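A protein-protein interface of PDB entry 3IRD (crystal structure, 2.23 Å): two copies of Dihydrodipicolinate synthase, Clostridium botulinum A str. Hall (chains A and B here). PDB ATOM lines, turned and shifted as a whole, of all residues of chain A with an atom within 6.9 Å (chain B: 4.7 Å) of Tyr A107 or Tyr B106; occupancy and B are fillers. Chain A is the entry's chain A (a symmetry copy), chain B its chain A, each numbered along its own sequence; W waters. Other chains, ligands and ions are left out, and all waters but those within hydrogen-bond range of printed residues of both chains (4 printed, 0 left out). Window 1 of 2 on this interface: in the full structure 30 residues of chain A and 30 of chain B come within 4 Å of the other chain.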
ATOM      1  N   THR A  49     -34.093   3.036 -32.385  1.00  0.00           N
ATOM      2  CA  THR A  49     -32.731   2.519 -32.458  1.00  0.00           C
ATOM      3  C   THR A  49     -32.498   1.554 -33.635  1.00  0.00           C
ATOM      4  O   THR A  49     -31.394   1.549 -34.233  1.00  0.00           O
ATOM      5  CB  THR A  49     -32.365   1.755 -31.224  1.00  0.00           C
ATOM      6  OG1 THR A  49     -32.407   2.607 -30.070  1.00  0.00           O
ATOM      7  CG2 THR A  49     -30.974   1.158 -31.397  1.00  0.00           C
ATOM      8  N   ASN A  80     -26.739   9.823 -28.229  1.00  0.00           N
ATOM      9  CA  ASN A  80     -25.595   9.925 -27.318  1.00  0.00           C
ATOM     10  C   ASN A  80     -24.405  10.690 -27.961  1.00  0.00           C
ATOM     11  O   ASN A  80     -23.370  10.931 -27.317  1.00  0.00           O
ATOM     12  CB  ASN A  80     -25.204   8.546 -26.767  1.00  0.00           C
ATOM     13  CG  ASN A  80     -24.782   7.549 -27.863  1.00  0.00           C
ATOM     14  OD1 ASN A  80     -25.022   7.772 -29.044  1.00  0.00           O
ATOM     15  ND2 ASN A  80     -24.127   6.447 -27.461  1.00  0.00           N
ATOM     16  N   PRO A 105     -27.336  11.544 -22.863  1.00  0.00           N
ATOM     17  CA  PRO A 105     -26.443  10.570 -23.478  1.00  0.00           C
ATOM     18  C   PRO A 105     -26.500   9.239 -22.694  1.00  0.00           C
ATOM     19  O   PRO A 105     -26.898   9.212 -21.529  1.00  0.00           O
ATOM     20  CB  PRO A 105     -25.061  11.205 -23.352  1.00  0.00           C
ATOM     21  CG  PRO A 105     -25.299  12.628 -23.195  1.00  0.00           C
ATOM     22  CD  PRO A 105     -26.651  12.811 -22.535  1.00  0.00           C
ATOM     23  N   TYR A 106     -26.099   8.151 -23.343  1.00  0.00           N
ATOM     24  CA  TYR A 106     -26.219   6.817 -22.733  1.00  0.00           C
ATOM     25  C   TYR A 106     -25.015   6.061 -23.225  1.00  0.00           C
ATOM     26  O   TYR A 106     -24.549   6.297 -24.356  1.00  0.00           O
ATOM     27  CB  TYR A 106     -27.521   6.120 -23.213  1.00  0.00           C
ATOM     28  CG  TYR A 106     -27.819   6.300 -24.687  1.00  0.00           C
ATOM     29  CD1 TYR A 106     -27.204   5.471 -25.658  1.00  0.00           C
ATOM     30  CD2 TYR A 106     -28.675   7.336 -25.127  1.00  0.00           C
ATOM     31  CE1 TYR A 106     -27.456   5.649 -27.037  1.00  0.00           C
ATOM     32  CE2 TYR A 106     -28.942   7.521 -26.476  1.00  0.00           C
ATOM     33  CZ  TYR A 106     -28.328   6.672 -27.430  1.00  0.00           C
ATOM     34  OH  TYR A 106     -28.572   6.882 -28.779  1.00  0.00           O
ATOM     35  N   TYR A 107     -24.536   5.124 -22.423  1.00  0.00           N
ATOM     36  CA  TYR A 107     -23.416   4.237 -22.844  1.00  0.00           C
ATOM     37  C   TYR A 107     -22.087   5.002 -22.848  1.00  0.00           C
ATOM     38  O   TYR A 107     -21.262   4.742 -21.950  1.00  0.00           O
ATOM     39  CB  TYR A 107     -23.681   3.488 -24.172  1.00  0.00           C
ATOM     40  CG  TYR A 107     -22.414   3.024 -24.892  1.00  0.00           C
ATOM     41  CD1 TYR A 107     -21.439   2.248 -24.226  1.00  0.00           C
ATOM     42  CD2 TYR A 107     -22.189   3.352 -26.234  1.00  0.00           C
ATOM     43  CE1 TYR A 107     -20.266   1.831 -24.860  1.00  0.00           C
ATOM     44  CE2 TYR A 107     -20.992   2.902 -26.912  1.00  0.00           C
ATOM     45  CZ  TYR A 107     -20.060   2.155 -26.210  1.00  0.00           C
ATOM     46  OH  TYR A 107     -18.899   1.749 -26.827  1.00  0.00           O
ATOM     47  N   ASN A 108     -21.896   5.962 -23.779  1.00  0.00           N
ATOM     48  CA  ASN A 108     -20.737   6.881 -23.632  1.00  0.00           C
ATOM     49  C   ASN A 108     -20.847   7.704 -22.351  1.00  0.00           C
ATOM     50  O   ASN A 108     -19.845   7.916 -21.653  1.00  0.00           O
ATOM     51  CB  ASN A 108     -20.383   7.739 -24.890  1.00  0.00           C
ATOM     52  CG  ASN A 108     -21.481   8.718 -25.301  1.00  0.00           C
ATOM     53  OD1 ASN A 108     -22.650   8.543 -24.968  1.00  0.00           O
ATOM     54  ND2 ASN A 108     -21.100   9.760 -26.060  1.00  0.00           N
ATOM     55  N   LYS A 109     -22.071   8.152 -22.053  1.00  0.00           N
ATOM     56  CA  LYS A 109     -22.373   8.943 -20.859  1.00  0.00           C
ATOM     57  C   LYS A 109     -21.587  10.259 -20.859  1.00  0.00           C
ATOM     58  O   LYS A 109     -21.088  10.646 -21.924  1.00  0.00           O
ATOM     59  CB  LYS A 109     -22.139   8.105 -19.605  1.00  0.00           C
ATOM     60  CG  LYS A 109     -22.957   6.804 -19.693  1.00  0.00           C
ATOM     61  CD  LYS A 109     -23.192   6.213 -18.342  1.00  0.00           C
ATOM     62  CE  LYS A 109     -21.906   5.807 -17.681  1.00  0.00           C
ATOM     63  NZ  LYS A 109     -22.138   5.715 -16.188  1.00  0.00           N
ATOM     64  N   THR A 110     -21.538  10.945 -19.700  1.00  0.00           N
ATOM     65  CA  THR A 110     -20.752  12.165 -19.477  1.00  0.00           C
ATOM     66  C   THR A 110     -20.991  12.638 -18.018  1.00  0.00           C
ATOM     67  O   THR A 110     -21.664  11.940 -17.258  1.00  0.00           O
ATOM     68  CB  THR A 110     -21.102  13.284 -20.500  1.00  0.00           C
ATOM     69  OG1 THR A 110     -20.199  14.389 -20.352  1.00  0.00           O
ATOM     70  CG2 THR A 110     -22.554  13.792 -20.362  1.00  0.00           C
ATOM     71  N   ARG A 138     -31.695   2.582 -18.381  1.00  0.00           N
ATOM     72  CA  ARG A 138     -31.354   2.300 -19.771  1.00  0.00           C
ATOM     73  C   ARG A 138     -30.019   2.934 -20.175  1.00  0.00           C
ATOM     74  O   ARG A 138     -29.250   2.305 -20.929  1.00  0.00           O
ATOM     75  CB  ARG A 138     -32.434   2.760 -20.768  1.00  0.00           C
ATOM     76  CG  ARG A 138     -33.750   1.978 -20.717  1.00  0.00           C
ATOM     77  CD  ARG A 138     -34.690   2.498 -21.835  1.00  0.00           C
ATOM     78  NE  ARG A 138     -35.919   1.706 -21.879  1.00  0.00           N
ATOM     79  CZ  ARG A 138     -36.079   0.540 -22.508  1.00  0.00           C
ATOM     80  NH1 ARG A 138     -37.242  -0.061 -22.427  1.00  0.00           N
ATOM     81  NH2 ARG A 138     -35.098  -0.046 -23.201  1.00  0.00           N
ATOM     82  N   THR A 139     -29.760   4.157 -19.693  1.00  0.00           N
ATOM     83  CA  THR A 139     -28.616   4.964 -20.131  1.00  0.00           C
ATOM     84  C   THR A 139     -27.366   4.768 -19.282  1.00  0.00           C
ATOM     85  O   THR A 139     -26.267   5.112 -19.708  1.00  0.00           O
ATOM     86  CB  THR A 139     -28.966   6.460 -20.147  1.00  0.00           C
ATOM     87  OG1 THR A 139     -29.124   6.955 -18.801  1.00  0.00           O
ATOM     88  CG2 THR A 139     -30.276   6.727 -21.024  1.00  0.00           C
ATOM     89  N   GLY A 140     -27.517   4.196 -18.087  1.00  0.00           N
ATOM     90  CA  GLY A 140     -26.413   4.203 -17.086  1.00  0.00           C
ATOM     91  C   GLY A 140     -26.178   5.572 -16.408  1.00  0.00           C
ATOM     92  O   GLY A 140     -25.266   5.740 -15.567  1.00  0.00           O
ATOM     93  N   LEU A 141     -27.006   6.560 -16.740  1.00  0.00           N
ATOM     94  CA  LEU A 141     -26.691   7.944 -16.390  1.00  0.00           C
ATOM     95  C   LEU A 141     -27.935   8.600 -15.847  1.00  0.00           C
ATOM     96  O   LEU A 141     -28.978   8.470 -16.471  1.00  0.00           O
ATOM     97  CB  LEU A 141     -26.152   8.715 -17.613  1.00  0.00           C
ATOM     98  CG  LEU A 141     -25.776  10.199 -17.498  1.00  0.00           C
ATOM     99  CD1 LEU A 141     -24.812  10.478 -16.321  1.00  0.00           C
ATOM    100  CD2 LEU A 141     -25.229  10.770 -18.805  1.00  0.00           C
ATOM    101  N   PRO A 269     -32.003  -6.108 -31.783  1.00  0.00           N
ATOM    102  CA  PRO A 269     -31.877  -7.235 -30.850  1.00  0.00           C
ATOM    103  C   PRO A 269     -33.089  -7.536 -29.977  1.00  0.00           C
ATOM    104  O   PRO A 269     -32.958  -8.407 -29.079  1.00  0.00           O
ATOM    105  CB  PRO A 269     -30.755  -6.806 -29.943  1.00  0.00           C
ATOM    106  CG  PRO A 269     -30.854  -5.295 -29.901  1.00  0.00           C
ATOM    107  CD  PRO A 269     -31.450  -4.856 -31.226  1.00  0.00           C
ATOM    108  N   THR B  44     -14.847   2.422 -26.622  1.00  0.00           N
ATOM    109  CA  THR B  44     -15.417   3.559 -25.897  1.00  0.00           C
ATOM    110  C   THR B  44     -14.370   4.623 -25.555  1.00  0.00           C
ATOM    111  O   THR B  44     -14.665   5.848 -25.544  1.00  0.00           O
ATOM    112  CB  THR B  44     -16.064   3.065 -24.568  1.00  0.00           C
ATOM    113  OG1 THR B  44     -16.757   1.820 -24.798  1.00  0.00           O
ATOM    114  CG2 THR B  44     -16.996   4.089 -23.981  1.00  0.00           C
ATOM    115  N   THR B  49     -18.474   6.764 -30.477  1.00  0.00           N
ATOM    116  CA  THR B  49     -19.831   7.298 -30.479  1.00  0.00           C
ATOM    117  C   THR B  49     -19.945   8.694 -31.120  1.00  0.00           C
ATOM    118  O   THR B  49     -20.966   8.998 -31.784  1.00  0.00           O
ATOM    119  CB  THR B  49     -20.370   7.441 -29.090  1.00  0.00           C
ATOM    120  OG1 THR B  49     -20.445   6.162 -28.443  1.00  0.00           O
ATOM    121  CG2 THR B  49     -21.745   8.093 -29.149  1.00  0.00           C
ATOM    122  N   SER B  79     -22.933  -2.249 -32.009  1.00  0.00           N
ATOM    123  CA  SER B  79     -23.825  -1.168 -31.619  1.00  0.00           C
ATOM    124  C   SER B  79     -25.108  -1.779 -31.051  1.00  0.00           C
ATOM    125  O   SER B  79     -25.180  -2.994 -30.851  1.00  0.00           O
ATOM    126  CB  SER B  79     -24.058  -0.188 -32.792  1.00  0.00           C
ATOM    127  OG  SER B  79     -25.213  -0.424 -33.582  1.00  0.00           O
ATOM    128  N   ASN B  80     -26.084  -0.946 -30.737  1.00  0.00           N
ATOM    129  CA  ASN B  80     -27.328  -1.411 -30.117  1.00  0.00           C
ATOM    130  C   ASN B  80     -28.407  -1.773 -31.175  1.00  0.00           C
ATOM    131  O   ASN B  80     -29.506  -2.246 -30.841  1.00  0.00           O
ATOM    132  CB  ASN B  80     -27.824  -0.412 -29.061  1.00  0.00           C
ATOM    133  CG  ASN B  80     -28.137   0.981 -29.639  1.00  0.00           C
ATOM    134  OD1 ASN B  80     -27.746   1.302 -30.755  1.00  0.00           O
ATOM    135  ND2 ASN B  80     -28.868   1.806 -28.872  1.00  0.00           N
ATOM    136  N   ILE B 103     -19.862  -4.972 -28.273  1.00  0.00           N
ATOM    137  CA  ILE B 103     -20.616  -4.673 -27.049  1.00  0.00           C
ATOM    138  C   ILE B 103     -22.041  -5.252 -27.115  1.00  0.00           C
ATOM    139  O   ILE B 103     -22.588  -5.447 -28.214  1.00  0.00           O
ATOM    140  CB  ILE B 103     -20.653  -3.147 -26.845  1.00  0.00           C
ATOM    141  CG1 ILE B 103     -21.127  -2.800 -25.430  1.00  0.00           C
ATOM    142  CG2 ILE B 103     -21.447  -2.476 -27.976  1.00  0.00           C
ATOM    143  CD1 ILE B 103     -20.737  -1.414 -24.978  1.00  0.00           C
ATOM    144  N   THR B 104     -22.603  -5.603 -25.947  1.00  0.00           N
ATOM    145  CA  THR B 104     -24.021  -5.946 -25.812  1.00  0.00           C
ATOM    146  C   THR B 104     -24.829  -4.709 -26.286  1.00  0.00           C
ATOM    147  O   THR B 104     -24.302  -3.614 -26.341  1.00  0.00           O
ATOM    148  CB  THR B 104     -24.424  -6.211 -24.346  1.00  0.00           C
ATOM    149  OG1 THR B 104     -24.258  -5.019 -23.584  1.00  0.00           O
ATOM    150  CG2 THR B 104     -23.639  -7.405 -23.703  1.00  0.00           C
ATOM    151  N   PRO B 105     -26.105  -4.900 -26.677  1.00  0.00           N
ATOM    152  CA  PRO B 105     -26.943  -3.728 -26.897  1.00  0.00           C
ATOM    153  C   PRO B 105     -27.023  -2.890 -25.602  1.00  0.00           C
ATOM    154  O   PRO B 105     -26.773  -3.397 -24.508  1.00  0.00           O
ATOM    155  CB  PRO B 105     -28.312  -4.311 -27.240  1.00  0.00           C
ATOM    156  CG  PRO B 105     -28.053  -5.661 -27.708  1.00  0.00           C
ATOM    157  CD  PRO B 105     -26.788  -6.159 -27.037  1.00  0.00           C
ATOM    158  N   TYR B 106     -27.372  -1.615 -25.740  1.00  0.00           N
ATOM    159  CA  TYR B 106     -27.368  -0.699 -24.588  1.00  0.00           C
ATOM    160  C   TYR B 106     -28.523   0.233 -24.835  1.00  0.00           C
ATOM    161  O   TYR B 106     -28.839   0.541 -26.001  1.00  0.00           O
ATOM    162  CB  TYR B 106     -26.037   0.101 -24.541  1.00  0.00           C
ATOM    163  CG  TYR B 106     -25.555   0.590 -25.891  1.00  0.00           C
ATOM    164  CD1 TYR B 106     -26.068   1.783 -26.457  1.00  0.00           C
ATOM    165  CD2 TYR B 106     -24.620  -0.165 -26.637  1.00  0.00           C
ATOM    166  CE1 TYR B 106     -25.642   2.232 -27.727  1.00  0.00           C
ATOM    167  CE2 TYR B 106     -24.183   0.264 -27.882  1.00  0.00           C
ATOM    168  CZ  TYR B 106     -24.699   1.468 -28.425  1.00  0.00           C
ATOM    169  OH  TYR B 106     -24.284   1.876 -29.684  1.00  0.00           O
ATOM    170  N   TYR B 107     -29.126   0.727 -23.766  1.00  0.00           N
ATOM    171  CA  TYR B 107     -30.210   1.740 -23.881  1.00  0.00           C
ATOM    172  C   TYR B 107     -31.505   1.097 -24.392  1.00  0.00           C
ATOM    173  O   TYR B 107     -32.442   0.952 -23.582  1.00  0.00           O
ATOM    174  CB  TYR B 107     -29.805   2.996 -24.691  1.00  0.00           C
ATOM    175  CG  TYR B 107     -30.986   3.769 -25.278  1.00  0.00           C
ATOM    176  CD1 TYR B 107     -32.059   4.194 -24.462  1.00  0.00           C
ATOM    177  CD2 TYR B 107     -31.033   4.082 -26.641  1.00  0.00           C
ATOM    178  CE1 TYR B 107     -33.155   4.884 -24.983  1.00  0.00           C
ATOM    179  CE2 TYR B 107     -32.150   4.822 -27.189  1.00  0.00           C
ATOM    180  CZ  TYR B 107     -33.184   5.204 -26.350  1.00  0.00           C
ATOM    181  OH  TYR B 107     -34.271   5.877 -26.859  1.00  0.00           O
ATOM    182  N   ASN B 108     -31.552   0.660 -25.668  1.00  0.00           N
ATOM    183  CA  ASN B 108     -32.693  -0.194 -26.092  1.00  0.00           C
ATOM    184  C   ASN B 108     -32.717  -1.505 -25.311  1.00  0.00           C
ATOM    185  O   ASN B 108     -33.792  -1.977 -24.911  1.00  0.00           O
ATOM    186  CB  ASN B 108     -32.862  -0.389 -27.634  1.00  0.00           C
ATOM    187  CG  ASN B 108     -31.694  -1.112 -28.299  1.00  0.00           C
ATOM    188  OD1 ASN B 108     -30.581  -1.139 -27.782  1.00  0.00           O
ATOM    189  ND2 ASN B 108     -31.947  -1.694 -29.485  1.00  0.00           N
ATOM    190  N   LYS B 109     -31.527  -2.075 -25.096  1.00  0.00           N
ATOM    191  CA  LYS B 109     -31.352  -3.324 -24.354  1.00  0.00           C
ATOM    192  C   LYS B 109     -32.094  -4.478 -25.039  1.00  0.00           C
ATOM    193  O   LYS B 109     -32.445  -4.334 -26.217  1.00  0.00           O
ATOM    194  CB  LYS B 109     -31.764  -3.128 -22.898  1.00  0.00           C
ATOM    195  CG  LYS B 109     -30.980  -1.949 -22.293  1.00  0.00           C
ATOM    196  CD  LYS B 109     -30.932  -2.031 -20.803  1.00  0.00           C
ATOM    197  CE  LYS B 109     -32.301  -1.926 -20.195  1.00  0.00           C
ATOM    198  NZ  LYS B 109     -32.259  -2.518 -18.802  1.00  0.00           N
ATOM    199  N   ARG B 138     -22.600   0.984 -18.162  1.00  0.00           N
ATOM    200  CA  ARG B 138     -22.774   1.866 -19.310  1.00  0.00           C
ATOM    201  C   ARG B 138     -24.030   1.519 -20.117  1.00  0.00           C
ATOM    202  O   ARG B 138     -24.718   2.442 -20.599  1.00  0.00           O
ATOM    203  CB  ARG B 138     -21.566   1.869 -20.266  1.00  0.00           C
ATOM    204  CG  ARG B 138     -20.289   2.508 -19.708  1.00  0.00           C
ATOM    205  CD  ARG B 138     -19.203   2.514 -20.815  1.00  0.00           C
ATOM    206  NE  ARG B 138     -18.003   3.205 -20.347  1.00  0.00           N
ATOM    207  CZ  ARG B 138     -17.800   4.525 -20.364  1.00  0.00           C
ATOM    208  NH1 ARG B 138     -16.674   4.992 -19.880  1.00  0.00           N
ATOM    209  NH2 ARG B 138     -18.704   5.387 -20.838  1.00  0.00           N
ATOM    210  N   THR B 139     -24.310   0.218 -20.268  1.00  0.00           N
ATOM    211  CA  THR B 139     -25.367  -0.274 -21.158  1.00  0.00           C
ATOM    212  C   THR B 139     -26.718  -0.441 -20.473  1.00  0.00           C
ATOM    213  O   THR B 139     -27.745  -0.527 -21.141  1.00  0.00           O
ATOM    214  CB  THR B 139     -24.974  -1.615 -21.797  1.00  0.00           C
ATOM    215  OG1 THR B 139     -24.969  -2.663 -20.807  1.00  0.00           O
ATOM    216  CG2 THR B 139     -23.558  -1.500 -22.531  1.00  0.00           C
HETATM  217  O   HOH W   1     -29.378   4.182 -30.158  1.00  0.00           O
HETATM  218  O   HOH W   2     -36.150  -1.320 -25.937  1.00  0.00           O
HETATM  219  O   HOH W   3     -17.360   7.718 -22.563  1.00  0.00           O
HETATM  220  O   HOH W   4     -23.393   4.882 -29.599  1.00  0.00           O
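Of chain B, only Thr B44 (3.0 Å), Thr B49 (3.6 Å), Ile B103 (3.3 Å), Tyr B106 (3.7 Å) and Arg B138 (2.9 Å) come within 4 Å of Tyr A107. Of the printed residues of chain A, Arg B138 touches Tyr A107, Asn A108 and Thr A139. Printed residues of chain A within 4 Å of Thr B139: Arg A138. Of the printed residues of chain B, Pro A269 touches Asn B80, Pro B105 and Asn B108. Printed residues of chain B within 4 Å of Thr A49: Asn B80, Tyr B107 and Asn B108. Of the printed residues of chain A, Asn B108 touches Thr A49, Arg A138 and Pro A269. Thr B104 touches none of the printed residues of chain A. The nearest printed residue of chain A that does not touch Tyr B106 is Arg A138 (4.5 Å). The nearest printed residue of chain B that does not touch Pro A269 is Lys B109 (4.1 Å).
Thr A49 touches Asn B80, and with the chains exchanged Asn A80 touches Thr B49. Thr A49 touches Tyr B107, and with the chains exchanged Tyr A107 touches Thr B49. Tyr B106 touches its own counterpart, Tyr A106. Tyr A107 touches Arg B138, and with the chains exchanged Arg A138 touches Tyr B107.
Among the printed residues, merely in contact across the chains: Thr A49 with Asn B80, Thr A49 with Tyr B107, Thr A49 with Asn B108, Asn A80 with Thr B49, Tyr A106 with Tyr B106, Tyr A106 with Tyr B107, Tyr A107 with Thr B49, Tyr A107 with Ile B103, Tyr A107 with Tyr B106, Asn A108 with Thr B49, Pro A269 with Asn B80, Pro A269 with Pro B105 and Pro A269 with Asn B108.
O of Asn B108 is in hydrogen-bond range of NH2 of Arg A138, 2.9 Å away. The backbone carbonyl oxygen (O) of Tyr B107 lies within hydrogen-bond range of the guanidinium group (NH2) of Arg A138 (2.9 Å). The backbone carbonyl oxygen (O) of Arg A138 sits close to the backbone carbonyl oxygen (O) of Thr B139 (3.2 Å). The guanidinium group of Arg B138 sits at hydrogen-bond distance from the backbone carbonyl oxygen of Asn A108, at 2.9 Å. The backbone carbonyl oxygen (O) of Tyr A107 is in hydrogen-bond range of the guanidinium group (NH2) of Arg B138, at 2.9 Å. The backbone carbonyl oxygen of Arg B138 sits close to the backbone carbonyl oxygen of Thr A139. OG1 of Thr B44 lies within hydrogen-bond range of OH of Tyr A107 (3.0 Å).
The backbone carbonyl oxygen (O) of Tyr A106 sits at hydrogen-bond distance from the side-chain amide nitrogen (ND2) of Asn A80 (3.1 Å). The side-chain amide nitrogen (ND2) of Asn B80 lies within hydrogen-bond range of the backbone carbonyl oxygen (O) of Tyr B106, at 3.1 Å. The backbone carbonyl oxygen (O) of Tyr A106 sits close to the side-chain amide oxygen (OD1) of Asn A108, at 3.0 Å. O of Asn A80 lies within hydrogen-bond range of ND2 of Asn A108 (2.8 Å). The backbone NH (N) of Tyr B107 sits at hydrogen-bond distance from the backbone carbonyl oxygen (O) of Thr B139 (3.2 Å). The backbone carbonyl oxygen (O) of Tyr B106 sits close to the side-chain amide oxygen (OD1) of Asn B108 (3.0 Å).
Water W2 lies within hydrogen-bond range of the backbone carbonyl oxygen of Asn B108 (2.7 Å) and the guanidinium group of Arg A138 (3.2 Å). Water W3 lies within hydrogen-bond range of O of Asn A108 (2.7 Å) and NH2 of Arg B138 (3.2 Å). Water W1 lies within hydrogen-bond range of ND2 of Asn B80 (2.7 Å), OH of Tyr A106 (3.1 Å) and OG1 of Thr A49 (3.4 Å). Water W4 lies within hydrogen-bond range of ND2 of Asn A80 (2.7 Å), OH of Tyr B106 (3.1 Å) and OG1 of Thr B49 (3.4 Å).
Hydrophobic or aromatic side chains of chain A that line the printed part of chain B: Tyr A106, Tyr A107 and Pro A269. Printed residues of chain B that touch a printed residue of chain A: Thr B44, Thr B49, Asn B80, Ile B103, Pro B105, Tyr B106, Tyr B107, Asn B108, Arg B138 and Thr B139. Hydrophobic or aromatic side chains of chain B within 4 Å of the printed part of chain A: Ile B103, Pro B105, Tyr B106 and Tyr B107. Among the printed residues, no Asp or Glu carboxylate lies within 4 Å of a Lys or Arg side-chain nitrogen of the other chain.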
